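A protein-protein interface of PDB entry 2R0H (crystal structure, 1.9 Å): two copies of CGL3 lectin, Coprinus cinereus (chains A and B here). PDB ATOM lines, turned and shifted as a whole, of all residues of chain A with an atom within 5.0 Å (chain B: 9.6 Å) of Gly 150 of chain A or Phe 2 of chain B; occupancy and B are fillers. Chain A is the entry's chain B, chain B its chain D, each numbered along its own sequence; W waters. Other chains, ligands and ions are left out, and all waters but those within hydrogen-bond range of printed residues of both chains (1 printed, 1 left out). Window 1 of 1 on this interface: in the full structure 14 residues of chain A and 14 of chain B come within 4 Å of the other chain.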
ATOM      1  N   PHE A   2      14.563  22.174  35.194  1.00  0.00           N
ATOM      2  CA  PHE A   2      13.677  22.618  34.130  1.00  0.00           C
ATOM      3  C   PHE A   2      12.597  23.634  34.519  1.00  0.00           C
ATOM      4  O   PHE A   2      12.020  23.581  35.600  1.00  0.00           O
ATOM      5  CB  PHE A   2      13.048  21.350  33.525  1.00  0.00           C
ATOM      6  CG  PHE A   2      12.153  21.607  32.369  1.00  0.00           C
ATOM      7  CD1 PHE A   2      12.687  21.783  31.111  1.00  0.00           C
ATOM      8  CD2 PHE A   2      10.775  21.606  32.517  1.00  0.00           C
ATOM      9  CE1 PHE A   2      11.866  22.013  30.028  1.00  0.00           C
ATOM     10  CE2 PHE A   2       9.953  21.832  31.434  1.00  0.00           C
ATOM     11  CZ  PHE A   2      10.498  22.019  30.190  1.00  0.00           C
ATOM     12  N   HIS A   3      12.312  24.547  33.603  1.00  0.00           N
ATOM     13  CA  HIS A   3      11.309  25.561  33.826  1.00  0.00           C
ATOM     14  C   HIS A   3      10.566  25.842  32.538  1.00  0.00           C
ATOM     15  O   HIS A   3      11.166  25.844  31.484  1.00  0.00           O
ATOM     16  CB  HIS A   3      11.985  26.908  34.185  1.00  0.00           C
ATOM     17  CG  HIS A   3      12.821  26.865  35.426  1.00  0.00           C
ATOM     18  ND1 HIS A   3      14.178  26.625  35.405  1.00  0.00           N
ATOM     19  CD2 HIS A   3      12.490  27.042  36.724  1.00  0.00           C
ATOM     20  CE1 HIS A   3      14.644  26.648  36.638  1.00  0.00           C
ATOM     21  NE2 HIS A   3      13.640  26.881  37.460  1.00  0.00           N
ATOM     22  N   VAL A  24      19.935  26.943  29.238  1.00  0.00           N
ATOM     23  CA  VAL A  24      19.519  26.580  27.874  1.00  0.00           C
ATOM     24  C   VAL A  24      18.058  26.927  27.616  1.00  0.00           C
ATOM     25  O   VAL A  24      17.175  26.452  28.341  1.00  0.00           O
ATOM     26  CB  VAL A  24      19.601  25.031  27.645  1.00  0.00           C
ATOM     27  CG1 VAL A  24      19.262  24.693  26.173  1.00  0.00           C
ATOM     28  CG2 VAL A  24      20.970  24.521  27.980  1.00  0.00           C
ATOM     29  N   PHE A  25      17.810  27.796  26.632  1.00  0.00           N
ATOM     30  CA  PHE A  25      16.448  28.191  26.234  1.00  0.00           C
ATOM     31  C   PHE A  25      16.124  27.346  25.020  1.00  0.00           C
ATOM     32  O   PHE A  25      16.761  27.524  23.986  1.00  0.00           O
ATOM     33  CB  PHE A  25      16.391  29.651  25.788  1.00  0.00           C
ATOM     34  CG  PHE A  25      16.626  30.630  26.885  1.00  0.00           C
ATOM     35  CD1 PHE A  25      15.549  31.166  27.575  1.00  0.00           C
ATOM     36  CD2 PHE A  25      17.896  31.053  27.188  1.00  0.00           C
ATOM     37  CE1 PHE A  25      15.753  32.108  28.569  1.00  0.00           C
ATOM     38  CE2 PHE A  25      18.110  31.943  28.215  1.00  0.00           C
ATOM     39  CZ  PHE A  25      17.027  32.478  28.892  1.00  0.00           C
ATOM     40  N   GLN A  26      15.130  26.466  25.134  1.00  0.00           N
ATOM     41  CA  GLN A  26      14.736  25.575  24.039  1.00  0.00           C
ATOM     42  C   GLN A  26      13.384  25.901  23.399  1.00  0.00           C
ATOM     43  O   GLN A  26      12.391  26.114  24.086  1.00  0.00           O
ATOM     44  CB  GLN A  26      14.731  24.112  24.491  1.00  0.00           C
ATOM     45  CG  GLN A  26      16.083  23.562  24.888  1.00  0.00           C
ATOM     46  CD  GLN A  26      16.081  22.054  24.999  1.00  0.00           C
ATOM     47  OE1 GLN A  26      15.916  21.350  24.004  1.00  0.00           O
ATOM     48  NE2 GLN A  26      16.267  21.550  26.209  1.00  0.00           N
ATOM     49  N   SER A  27      13.362  25.910  22.071  1.00  0.00           N
ATOM     50  CA  SER A  27      12.161  26.183  21.298  1.00  0.00           C
ATOM     51  C   SER A  27      11.829  24.917  20.499  1.00  0.00           C
ATOM     52  O   SER A  27      12.727  24.132  20.180  1.00  0.00           O
ATOM     53  CB  SER A  27      12.445  27.308  20.295  1.00  0.00           C
ATOM     54  OG  SER A  27      11.351  27.512  19.392  1.00  0.00           O
ATOM     55  N   ASP A  28      10.563  24.672  20.222  1.00  0.00           N
ATOM     56  CA  ASP A  28      10.261  23.510  19.414  1.00  0.00           C
ATOM     57  C   ASP A  28       9.949  23.963  18.007  1.00  0.00           C
ATOM     58  O   ASP A  28       9.466  23.189  17.190  1.00  0.00           O
ATOM     59  CB  ASP A  28       9.162  22.634  20.021  1.00  0.00           C
ATOM     60  CG  ASP A  28       7.778  23.222  19.857  1.00  0.00           C
ATOM     61  OD1 ASP A  28       7.663  24.423  19.551  1.00  0.00           O
ATOM     62  OD2 ASP A  28       6.802  22.467  20.036  1.00  0.00           O
ATOM     63  N   ASP A  98      14.329  22.474  16.229  1.00  0.00           N
ATOM     64  CA  ASP A  98      14.087  22.854  17.613  1.00  0.00           C
ATOM     65  C   ASP A  98      15.285  23.645  18.101  1.00  0.00           C
ATOM     66  O   ASP A  98      16.172  23.103  18.758  1.00  0.00           O
ATOM     67  CB  ASP A  98      13.898  21.609  18.480  1.00  0.00           C
ATOM     68  CG  ASP A  98      15.073  20.651  18.390  1.00  0.00           C
ATOM     69  OD1 ASP A  98      15.779  20.665  17.363  1.00  0.00           O
ATOM     70  OD2 ASP A  98      15.285  19.879  19.347  1.00  0.00           O
ATOM     71  N   VAL A 148       6.269  29.139  23.914  1.00  0.00           N
ATOM     72  CA  VAL A 148       6.607  28.603  25.226  1.00  0.00           C
ATOM     73  C   VAL A 148       7.984  27.958  24.987  1.00  0.00           C
ATOM     74  O   VAL A 148       8.168  27.231  23.996  1.00  0.00           O
ATOM     75  CB  VAL A 148       5.678  27.446  25.713  1.00  0.00           C
ATOM     76  CG1 VAL A 148       6.283  26.812  27.051  1.00  0.00           C
ATOM     77  CG2 VAL A 148       4.234  27.910  25.918  1.00  0.00           C
ATOM     78  N   LEU A 149       8.939  28.231  25.869  1.00  0.00           N
ATOM     79  CA  LEU A 149      10.270  27.655  25.758  1.00  0.00           C
ATOM     80  C   LEU A 149      10.535  26.744  26.957  1.00  0.00           C
ATOM     81  O   LEU A 149       9.940  26.916  28.010  1.00  0.00           O
ATOM     82  CB  LEU A 149      11.299  28.778  25.859  1.00  0.00           C
ATOM     83  CG  LEU A 149      11.109  29.875  24.813  1.00  0.00           C
ATOM     84  CD1 LEU A 149      12.163  30.975  25.021  1.00  0.00           C
ATOM     85  CD2 LEU A 149      11.176  29.258  23.405  1.00  0.00           C
ATOM     86  N   GLY A 150      11.381  25.745  26.770  1.00  0.00           N
ATOM     87  CA  GLY A 150      11.807  24.913  27.874  1.00  0.00           C
ATOM     88  C   GLY A 150      13.117  25.506  28.330  1.00  0.00           C
ATOM     89  O   GLY A 150      14.015  25.706  27.515  1.00  0.00           O
ATOM     90  N   VAL A 151      13.240  25.829  29.611  1.00  0.00           N
ATOM     91  CA  VAL A 151      14.493  26.439  30.036  1.00  0.00           C
ATOM     92  C   VAL A 151      15.141  25.501  31.033  1.00  0.00           C
ATOM     93  O   VAL A 151      14.509  25.099  31.995  1.00  0.00           O
ATOM     94  CB  VAL A 151      14.326  27.805  30.703  1.00  0.00           C
ATOM     95  CG1 VAL A 151      15.682  28.368  31.098  1.00  0.00           C
ATOM     96  CG2 VAL A 151      13.636  28.796  29.789  1.00  0.00           C
ATOM     97  N   THR A 152      16.362  25.079  30.739  1.00  0.00           N
ATOM     98  CA  THR A 152      17.083  24.187  31.628  1.00  0.00           C
ATOM     99  C   THR A 152      18.283  24.895  32.205  1.00  0.00           C
ATOM    100  O   THR A 152      19.092  25.515  31.479  1.00  0.00           O
ATOM    101  CB  THR A 152      17.558  22.895  30.902  1.00  0.00           C
ATOM    102  OG1 THR A 152      16.422  22.206  30.353  1.00  0.00           O
ATOM    103  CG2 THR A 152      18.290  21.962  31.880  1.00  0.00           C
ATOM    104  N   MET B   1      15.500  15.854  20.126  1.00  0.00           N
ATOM    105  CA  MET B   1      14.424  16.641  19.536  1.00  0.00           C
ATOM    106  C   MET B   1      13.384  17.047  20.577  1.00  0.00           C
ATOM    107  O   MET B   1      12.774  16.209  21.218  1.00  0.00           O
ATOM    108  CB  MET B   1      13.757  15.875  18.408  1.00  0.00           C
ATOM    109  CG  MET B   1      12.610  16.625  17.781  1.00  0.00           C
ATOM    110  SD  MET B   1      13.098  18.251  17.194  1.00  0.00           S
ATOM    111  CE  MET B   1      13.154  17.978  15.421  1.00  0.00           C
ATOM    112  N   PHE B   2      13.199  18.348  20.717  1.00  0.00           N
ATOM    113  CA  PHE B   2      12.345  18.919  21.738  1.00  0.00           C
ATOM    114  C   PHE B   2      10.971  19.368  21.237  1.00  0.00           C
ATOM    115  O   PHE B   2      10.846  19.937  20.141  1.00  0.00           O
ATOM    116  CB  PHE B   2      13.090  20.085  22.382  1.00  0.00           C
ATOM    117  CG  PHE B   2      12.301  20.809  23.439  1.00  0.00           C
ATOM    118  CD1 PHE B   2      12.317  20.383  24.754  1.00  0.00           C
ATOM    119  CD2 PHE B   2      11.581  21.926  23.118  1.00  0.00           C
ATOM    120  CE1 PHE B   2      11.606  21.062  25.726  1.00  0.00           C
ATOM    121  CE2 PHE B   2      10.869  22.609  24.077  1.00  0.00           C
ATOM    122  CZ  PHE B   2      10.883  22.164  25.389  1.00  0.00           C
ATOM    123  N   HIS B   3       9.945  19.086  22.040  1.00  0.00           N
ATOM    124  CA  HIS B   3       8.588  19.458  21.717  1.00  0.00           C
ATOM    125  C   HIS B   3       7.839  20.054  22.910  1.00  0.00           C
ATOM    126  O   HIS B   3       8.069  19.648  24.032  1.00  0.00           O
ATOM    127  CB  HIS B   3       7.795  18.235  21.264  1.00  0.00           C
ATOM    128  CG  HIS B   3       8.346  17.540  20.058  1.00  0.00           C
ATOM    129  ND1 HIS B   3       9.207  16.462  20.142  1.00  0.00           N
ATOM    130  CD2 HIS B   3       8.111  17.729  18.740  1.00  0.00           C
ATOM    131  CE1 HIS B   3       9.507  16.042  18.926  1.00  0.00           C
ATOM    132  NE2 HIS B   3       8.860  16.797  18.057  1.00  0.00           N
ATOM    133  N   ILE B   4       6.966  21.034  22.660  1.00  0.00           N
ATOM    134  CA  ILE B   4       6.159  21.645  23.709  1.00  0.00           C
ATOM    135  C   ILE B   4       4.850  20.861  23.674  1.00  0.00           C
ATOM    136  O   ILE B   4       4.257  20.663  22.609  1.00  0.00           O
ATOM    137  CB  ILE B   4       5.841  23.125  23.425  1.00  0.00           C
ATOM    138  CG1 ILE B   4       7.122  23.991  23.536  1.00  0.00           C
ATOM    139  CG2 ILE B   4       4.824  23.638  24.418  1.00  0.00           C
ATOM    140  CD1 ILE B   4       7.764  24.016  24.908  1.00  0.00           C
ATOM    141  N   LEU B   5       4.421  20.366  24.830  1.00  0.00           N
ATOM    142  CA  LEU B   5       3.179  19.612  24.897  1.00  0.00           C
ATOM    143  C   LEU B   5       2.258  20.245  25.929  1.00  0.00           C
ATOM    144  O   LEU B   5       2.470  20.083  27.119  1.00  0.00           O
ATOM    145  CB  LEU B   5       3.451  18.164  25.297  1.00  0.00           C
ATOM    146  CG  LEU B   5       2.231  17.225  25.452  1.00  0.00           C
ATOM    147  CD1 LEU B   5       1.362  17.135  24.191  1.00  0.00           C
ATOM    148  CD2 LEU B   5       2.754  15.839  25.847  1.00  0.00           C
ATOM    149  N   VAL B  11       0.777  16.159  20.344  1.00  0.00           N
ATOM    150  CA  VAL B  11       1.815  16.744  19.514  1.00  0.00           C
ATOM    151  C   VAL B  11       2.462  15.649  18.697  1.00  0.00           C
ATOM    152  O   VAL B  11       2.748  14.575  19.211  1.00  0.00           O
ATOM    153  CB  VAL B  11       2.925  17.429  20.328  1.00  0.00           C
ATOM    154  CG1 VAL B  11       2.365  18.600  21.140  1.00  0.00           C
ATOM    155  CG2 VAL B  11       3.654  16.413  21.223  1.00  0.00           C
ATOM    156  N   ASP B  12       2.691  15.922  17.419  1.00  0.00           N
ATOM    157  CA  ASP B  12       3.325  14.936  16.554  1.00  0.00           C
ATOM    158  C   ASP B  12       4.817  14.887  16.815  1.00  0.00           C
ATOM    159  O   ASP B  12       5.447  15.921  17.042  1.00  0.00           O
ATOM    160  CB  ASP B  12       3.164  15.359  15.085  1.00  0.00           C
ATOM    161  CG  ASP B  12       1.739  15.307  14.608  1.00  0.00           C
ATOM    162  OD1 ASP B  12       0.899  14.720  15.313  1.00  0.00           O
ATOM    163  OD2 ASP B  12       1.480  15.766  13.475  1.00  0.00           O
ATOM    164  N   LEU B  13       5.390  13.698  16.854  1.00  0.00           N
ATOM    165  CA  LEU B  13       6.828  13.630  16.967  1.00  0.00           C
ATOM    166  C   LEU B  13       7.327  14.067  15.600  1.00  0.00           C
ATOM    167  O   LEU B  13       6.582  14.024  14.625  1.00  0.00           O
ATOM    168  CB  LEU B  13       7.296  12.218  17.315  1.00  0.00           C
ATOM    169  CG  LEU B  13       6.807  11.714  18.675  1.00  0.00           C
ATOM    170  CD1 LEU B  13       7.471  10.404  19.035  1.00  0.00           C
ATOM    171  CD2 LEU B  13       7.049  12.754  19.754  1.00  0.00           C
ATOM    172  N   SER B  14       8.567  14.520  15.528  1.00  0.00           N
ATOM    173  CA  SER B  14       9.124  14.940  14.226  1.00  0.00           C
ATOM    174  C   SER B  14       9.194  13.772  13.240  1.00  0.00           C
ATOM    175  O   SER B  14       9.138  13.958  12.028  1.00  0.00           O
ATOM    176  CB  SER B  14      10.512  15.533  14.430  1.00  0.00           C
ATOM    177  OG  SER B  14      11.353  14.577  15.050  1.00  0.00           O
ATOM    178  N   ILE B  22      14.098   6.992  23.265  1.00  0.00           N
ATOM    179  CA  ILE B  22      13.830   7.397  24.652  1.00  0.00           C
ATOM    180  C   ILE B  22      12.993   8.661  24.586  1.00  0.00           C
ATOM    181  O   ILE B  22      13.370   9.610  23.902  1.00  0.00           O
ATOM    182  CB  ILE B  22      15.117   7.756  25.363  1.00  0.00           C
ATOM    183  CG1 ILE B  22      16.049   6.523  25.379  1.00  0.00           C
ATOM    184  CG2 ILE B  22      14.823   8.237  26.824  1.00  0.00           C
ATOM    185  CD1 ILE B  22      17.398   6.819  25.915  1.00  0.00           C
ATOM    186  N   ILE B  23      11.848   8.661  25.268  1.00  0.00           N
ATOM    187  CA  ILE B  23      10.980   9.837  25.278  1.00  0.00           C
ATOM    188  C   ILE B  23      10.879  10.278  26.705  1.00  0.00           C
ATOM    189  O   ILE B  23      10.509   9.467  27.557  1.00  0.00           O
ATOM    190  CB  ILE B  23       9.549   9.529  24.813  1.00  0.00           C
ATOM    191  CG1 ILE B  23       9.552   9.016  23.376  1.00  0.00           C
ATOM    192  CG2 ILE B  23       8.687  10.816  24.926  1.00  0.00           C
ATOM    193  CD1 ILE B  23       8.194   8.600  22.878  1.00  0.00           C
ATOM    194  N   VAL B  24      11.244  11.537  26.952  1.00  0.00           N
ATOM    195  CA  VAL B  24      11.215  12.143  28.293  1.00  0.00           C
ATOM    196  C   VAL B  24      10.188  13.274  28.383  1.00  0.00           C
ATOM    197  O   VAL B  24      10.286  14.272  27.661  1.00  0.00           O
ATOM    198  CB  VAL B  24      12.571  12.822  28.621  1.00  0.00           C
ATOM    199  CG1 VAL B  24      12.565  13.372  30.061  1.00  0.00           C
ATOM    200  CG2 VAL B  24      13.695  11.847  28.459  1.00  0.00           C
ATOM    201  N   PHE B  25       9.191  13.097  29.240  1.00  0.00           N
ATOM    202  CA  PHE B  25       8.141  14.110  29.467  1.00  0.00           C
ATOM    203  C   PHE B  25       8.624  14.872  30.680  1.00  0.00           C
ATOM    204  O   PHE B  25       8.756  14.281  31.763  1.00  0.00           O
ATOM    205  CB  PHE B  25       6.786  13.472  29.832  1.00  0.00           C
ATOM    206  CG  PHE B  25       6.130  12.713  28.717  1.00  0.00           C
ATOM    207  CD1 PHE B  25       5.185  13.340  27.919  1.00  0.00           C
ATOM    208  CD2 PHE B  25       6.431  11.372  28.476  1.00  0.00           C
ATOM    209  CE1 PHE B  25       4.570  12.667  26.872  1.00  0.00           C
ATOM    210  CE2 PHE B  25       5.812  10.694  27.429  1.00  0.00           C
ATOM    211  CZ  PHE B  25       4.874  11.351  26.629  1.00  0.00           C
ATOM    212  N   GLN B  26       8.870  16.166  30.522  1.00  0.00           N
ATOM    213  CA  GLN B  26       9.343  16.994  31.642  1.00  0.00           C
ATOM    214  C   GLN B  26       8.368  18.055  32.115  1.00  0.00           C
ATOM    215  O   GLN B  26       7.856  18.839  31.317  1.00  0.00           O
ATOM    216  CB  GLN B  26      10.714  17.658  31.361  1.00  0.00           C
ATOM    217  CG  GLN B  26      11.888  16.697  31.211  1.00  0.00           C
ATOM    218  CD  GLN B  26      13.220  17.406  30.974  1.00  0.00           C
ATOM    219  OE1 GLN B  26      13.288  18.633  30.934  1.00  0.00           O
ATOM    220  NE2 GLN B  26      14.285  16.628  30.827  1.00  0.00           N
ATOM    221  N   SER B  27       8.178  18.085  33.436  1.00  0.00           N
ATOM    222  CA  SER B  27       7.294  19.022  34.114  1.00  0.00           C
ATOM    223  C   SER B  27       8.139  19.959  34.974  1.00  0.00           C
ATOM    224  O   SER B  27       9.212  19.561  35.401  1.00  0.00           O
ATOM    225  CB  SER B  27       6.394  18.259  35.078  1.00  0.00           C
ATOM    226  OG  SER B  27       5.605  19.148  35.861  1.00  0.00           O
ATOM    227  N   ASP B  28       7.714  21.194  35.186  1.00  0.00           N
ATOM    228  CA  ASP B  28       8.491  22.052  36.062  1.00  0.00           C
ATOM    229  C   ASP B  28       7.841  22.126  37.425  1.00  0.00           C
ATOM    230  O   ASP B  28       8.246  22.906  38.281  1.00  0.00           O
ATOM    231  CB  ASP B  28       8.786  23.426  35.457  1.00  0.00           C
ATOM    232  CG  ASP B  28       7.583  24.349  35.451  1.00  0.00           C
ATOM    233  OD1 ASP B  28       6.488  23.918  35.859  1.00  0.00           O
ATOM    234  OD2 ASP B  28       7.748  25.512  35.034  1.00  0.00           O
ATOM    235  N   VAL B 133       2.367  12.091  20.873  1.00  0.00           N
ATOM    236  CA  VAL B 133       2.269  11.958  22.353  1.00  0.00           C
ATOM    237  C   VAL B 133       1.181  12.899  22.835  1.00  0.00           C
ATOM    238  O   VAL B 133       0.948  13.942  22.224  1.00  0.00           O
ATOM    239  CB  VAL B 133       3.591  12.171  23.115  1.00  0.00           C
ATOM    240  CG1 VAL B 133       4.630  11.087  22.734  1.00  0.00           C
ATOM    241  CG2 VAL B 133       4.166  13.575  22.857  1.00  0.00           C
ATOM    242  N   VAL B 148       2.125  22.640  30.950  1.00  0.00           N
ATOM    243  CA  VAL B 148       2.926  22.524  29.730  1.00  0.00           C
ATOM    244  C   VAL B 148       4.115  21.645  30.127  1.00  0.00           C
ATOM    245  O   VAL B 148       4.757  21.836  31.176  1.00  0.00           O
ATOM    246  CB  VAL B 148       3.492  23.855  29.127  1.00  0.00           C
ATOM    247  CG1 VAL B 148       4.281  23.506  27.869  1.00  0.00           C
ATOM    248  CG2 VAL B 148       2.372  24.840  28.780  1.00  0.00           C
ATOM    249  N   LEU B 149       4.398  20.685  29.269  1.00  0.00           N
ATOM    250  CA  LEU B 149       5.499  19.764  29.471  1.00  0.00           C
ATOM    251  C   LEU B 149       6.474  19.898  28.309  1.00  0.00           C
ATOM    252  O   LEU B 149       6.075  20.177  27.161  1.00  0.00           O
ATOM    253  CB  LEU B 149       4.984  18.315  29.404  1.00  0.00           C
ATOM    254  CG  LEU B 149       3.938  17.871  30.412  1.00  0.00           C
ATOM    255  CD1 LEU B 149       3.476  16.448  30.082  1.00  0.00           C
ATOM    256  CD2 LEU B 149       4.473  17.948  31.807  1.00  0.00           C
ATOM    257  N   GLY B 150       7.749  19.706  28.615  1.00  0.00           N
ATOM    258  CA  GLY B 150       8.775  19.621  27.601  1.00  0.00           C
ATOM    259  C   GLY B 150       8.967  18.151  27.306  1.00  0.00           C
ATOM    260  O   GLY B 150       9.193  17.357  28.211  1.00  0.00           O
ATOM    261  N   VAL B 151       8.851  17.783  26.041  1.00  0.00           N
ATOM    262  CA  VAL B 151       8.989  16.402  25.657  1.00  0.00           C
ATOM    263  C   VAL B 151      10.219  16.337  24.777  1.00  0.00           C
ATOM    264  O   VAL B 151      10.303  17.056  23.777  1.00  0.00           O
ATOM    265  CB  VAL B 151       7.787  15.891  24.816  1.00  0.00           C
ATOM    266  CG1 VAL B 151       8.062  14.460  24.353  1.00  0.00           C
ATOM    267  CG2 VAL B 151       6.470  15.984  25.573  1.00  0.00           C
ATOM    268  N   THR B 152      11.159  15.479  25.151  1.00  0.00           N
ATOM    269  CA  THR B 152      12.390  15.323  24.411  1.00  0.00           C
ATOM    270  C   THR B 152      12.586  13.881  23.958  1.00  0.00           C
ATOM    271  O   THR B 152      12.446  12.960  24.765  1.00  0.00           O
ATOM    272  CB  THR B 152      13.594  15.663  25.323  1.00  0.00           C
ATOM    273  OG1 THR B 152      13.485  17.007  25.837  1.00  0.00           O
ATOM    274  CG2 THR B 152      14.904  15.491  24.576  1.00  0.00           C
ATOM    275  N   VAL B 153      12.879  13.693  22.670  1.00  0.00           N
ATOM    276  CA  VAL B 153      13.127  12.356  22.127  1.00  0.00           C
ATOM    277  C   VAL B 153      14.644  12.231  21.947  1.00  0.00           C
ATOM    278  O   VAL B 153      15.301  13.095  21.364  1.00  0.00           O
ATOM    279  CB  VAL B 153      12.414  12.101  20.767  1.00  0.00           C
ATOM    280  CG1 VAL B 153      12.799  10.736  20.216  1.00  0.00           C
ATOM    281  CG2 VAL B 153      10.917  12.151  20.947  1.00  0.00           C
ATOM    282  N   LEU B 154      15.220  11.192  22.502  1.00  0.00           N
ATOM    283  CA  LEU B 154      16.640  11.011  22.369  1.00  0.00           C
ATOM    284  C   LEU B 154      17.014   9.549  22.275  1.00  0.00           C
ATOM    285  O   LEU B 154      16.163   8.672  22.408  1.00  0.00           O
ATOM    286  CB  LEU B 154      17.368  11.769  23.480  1.00  0.00           C
ATOM    287  CG  LEU B 154      16.980  11.474  24.925  1.00  0.00           C
ATOM    288  CD1 LEU B 154      17.302  10.051  25.315  1.00  0.00           C
ATOM    289  CD2 LEU B 154      17.625  12.485  25.869  1.00  0.00           C
ATOM    290  N   ASN B 158      23.223   9.648  21.949  1.00  0.00           N
ATOM    291  CA  ASN B 158      23.306  11.131  21.890  1.00  0.00           C
ATOM    292  C   ASN B 158      24.303  11.838  22.824  1.00  0.00           C
ATOM    293  O   ASN B 158      25.150  12.576  22.318  1.00  0.00           O
ATOM    294  CB  ASN B 158      21.926  11.825  21.882  1.00  0.00           C
ATOM    295  CG  ASN B 158      21.108  11.506  20.639  1.00  0.00           C
ATOM    296  OD1 ASN B 158      21.649  11.115  19.604  1.00  0.00           O
ATOM    297  ND2 ASN B 158      19.808  11.765  20.711  1.00  0.00           N
HETATM  298  O   HOH W   1      15.842  19.867  30.055  1.00  0.00           O
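Of the 13 printed residues of chain A, 8 touch a printed residue of chain B. Of the 25 printed residues of chain B, 9 touch a printed residue of chain A. Printed residues of chain B that touch a printed residue of chain A: Met 1, Phe 2, His 3, Ile 4, Gln 26, Ser 27, Asp 28, Val 148 and Gly 150.
Phe 2 of chain A touches Gln 26 of chain B, and with the chains exchanged Gln 26 of chain A touches Phe 2 of chain B. Phe 2 of chain A touches Asp 28 of chain B, and with the chains exchanged Asp 28 of chain A touches Phe 2 of chain B. His 3 of chain A touches Asp 28 of chain B, and with the chains exchanged Asp 28 of chain A touches His 3 of chain B. Val 148 of chain A touches its own counterpart, Val 148 of chain B. Of the 15 pairs that touch across the chains among the printed residues, 11 have their exchanged pair printed and touching as well.
OE1 of Gln 26 of chain B touches CD1 of Phe 2 of chain A, 3.2 Å away. Ser 27 of chain B touches Phe 2 of chain A (O to CD2, 3.9 Å). His 3 of chain A touches Asp 28 of chain B (CA to CB, 3.7 Å). CB of Phe 2 of chain B touches OE1 of Gln 26 of chain A, at 3.5 Å. Phe 2 of chain B touches Ser 27 of chain A (CD2 to O, 3.8 Å). O of Phe 2 of chain B touches CB of Asp 28 of chain A, 3.2 Å away. His 3 of chain B touches Asp 28 of chain A. Val 148 of chain A touches Ile 4 of chain B. Val 148 of chain B touches Val 148 of chain A. Gly 150 of chain A touches Phe 2 of chain B (CA to CZ, 3.8 Å).
N of Gln 26 of chain A lies within hydrogen-bond range of O of Gly 150 of chain A, 2.7 Å away. The backbone carbonyl oxygen (O) of Val 151 of chain B lies within hydrogen-bond range of the backbone NH (N) of His 3 of chain B. O of Met 1 of chain B is in hydrogen-bond range of N of Val 153 of chain B, 2.9 Å away. O of Gly 150 of chain B lies within hydrogen-bond range of N of Gln 26 of chain B (2.6 Å). The backbone NH of His 3 of chain A is in hydrogen-bond range of the backbone carbonyl oxygen of Val 151 of chain A (2.8 Å). N of Ser 14 of chain B sits at hydrogen-bond distance from NE2 of His 3 of chain B (3.4 Å).
Printed residues of chain B within 4 Å of His 3 of chain A: Asp 28. Gln 26 of chain A touches just one residue of chain B: Phe 2. Asp 28 of chain A touches just these residues of chain B: Phe 2, His 3 and Ile 4. No residue of chain B comes within 4 Å of Val 151 of chain A. Phe 2 of chain B touches five residues of chain A. Ser 14 of chain B touches none of the printed residues of chain A. Printed residues of chain A within 4 Å of Ser 27 of chain B: Phe 2 (3.9 Å). Of the printed residues of chain A, Asp 28 of chain B touches Phe 2 and His 3. Leu 154 of chain B touches none of the printed residues of chain A.
The side-chain carboxylate (OD2) of Asp 98 of chain A is in hydrogen-bond range of the backbone NH (N) of Phe 2 of chain B (2.9 Å). The side-chain carboxylate of Asp 28 of chain A lies within hydrogen-bond range of the backbone NH of Ile 4 of chain B, 3.0 Å away. OD2 of Asp 98 of chain A lies close to SD of Met 1 of chain B (3.5 Å).
Water W1 bridges the side-chain hydroxyl (OG1) of Thr 152 of chain A (2.4 Å) and the side-chain amide oxygen (OE1) of Gln 26 of chain B (3.0 Å).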
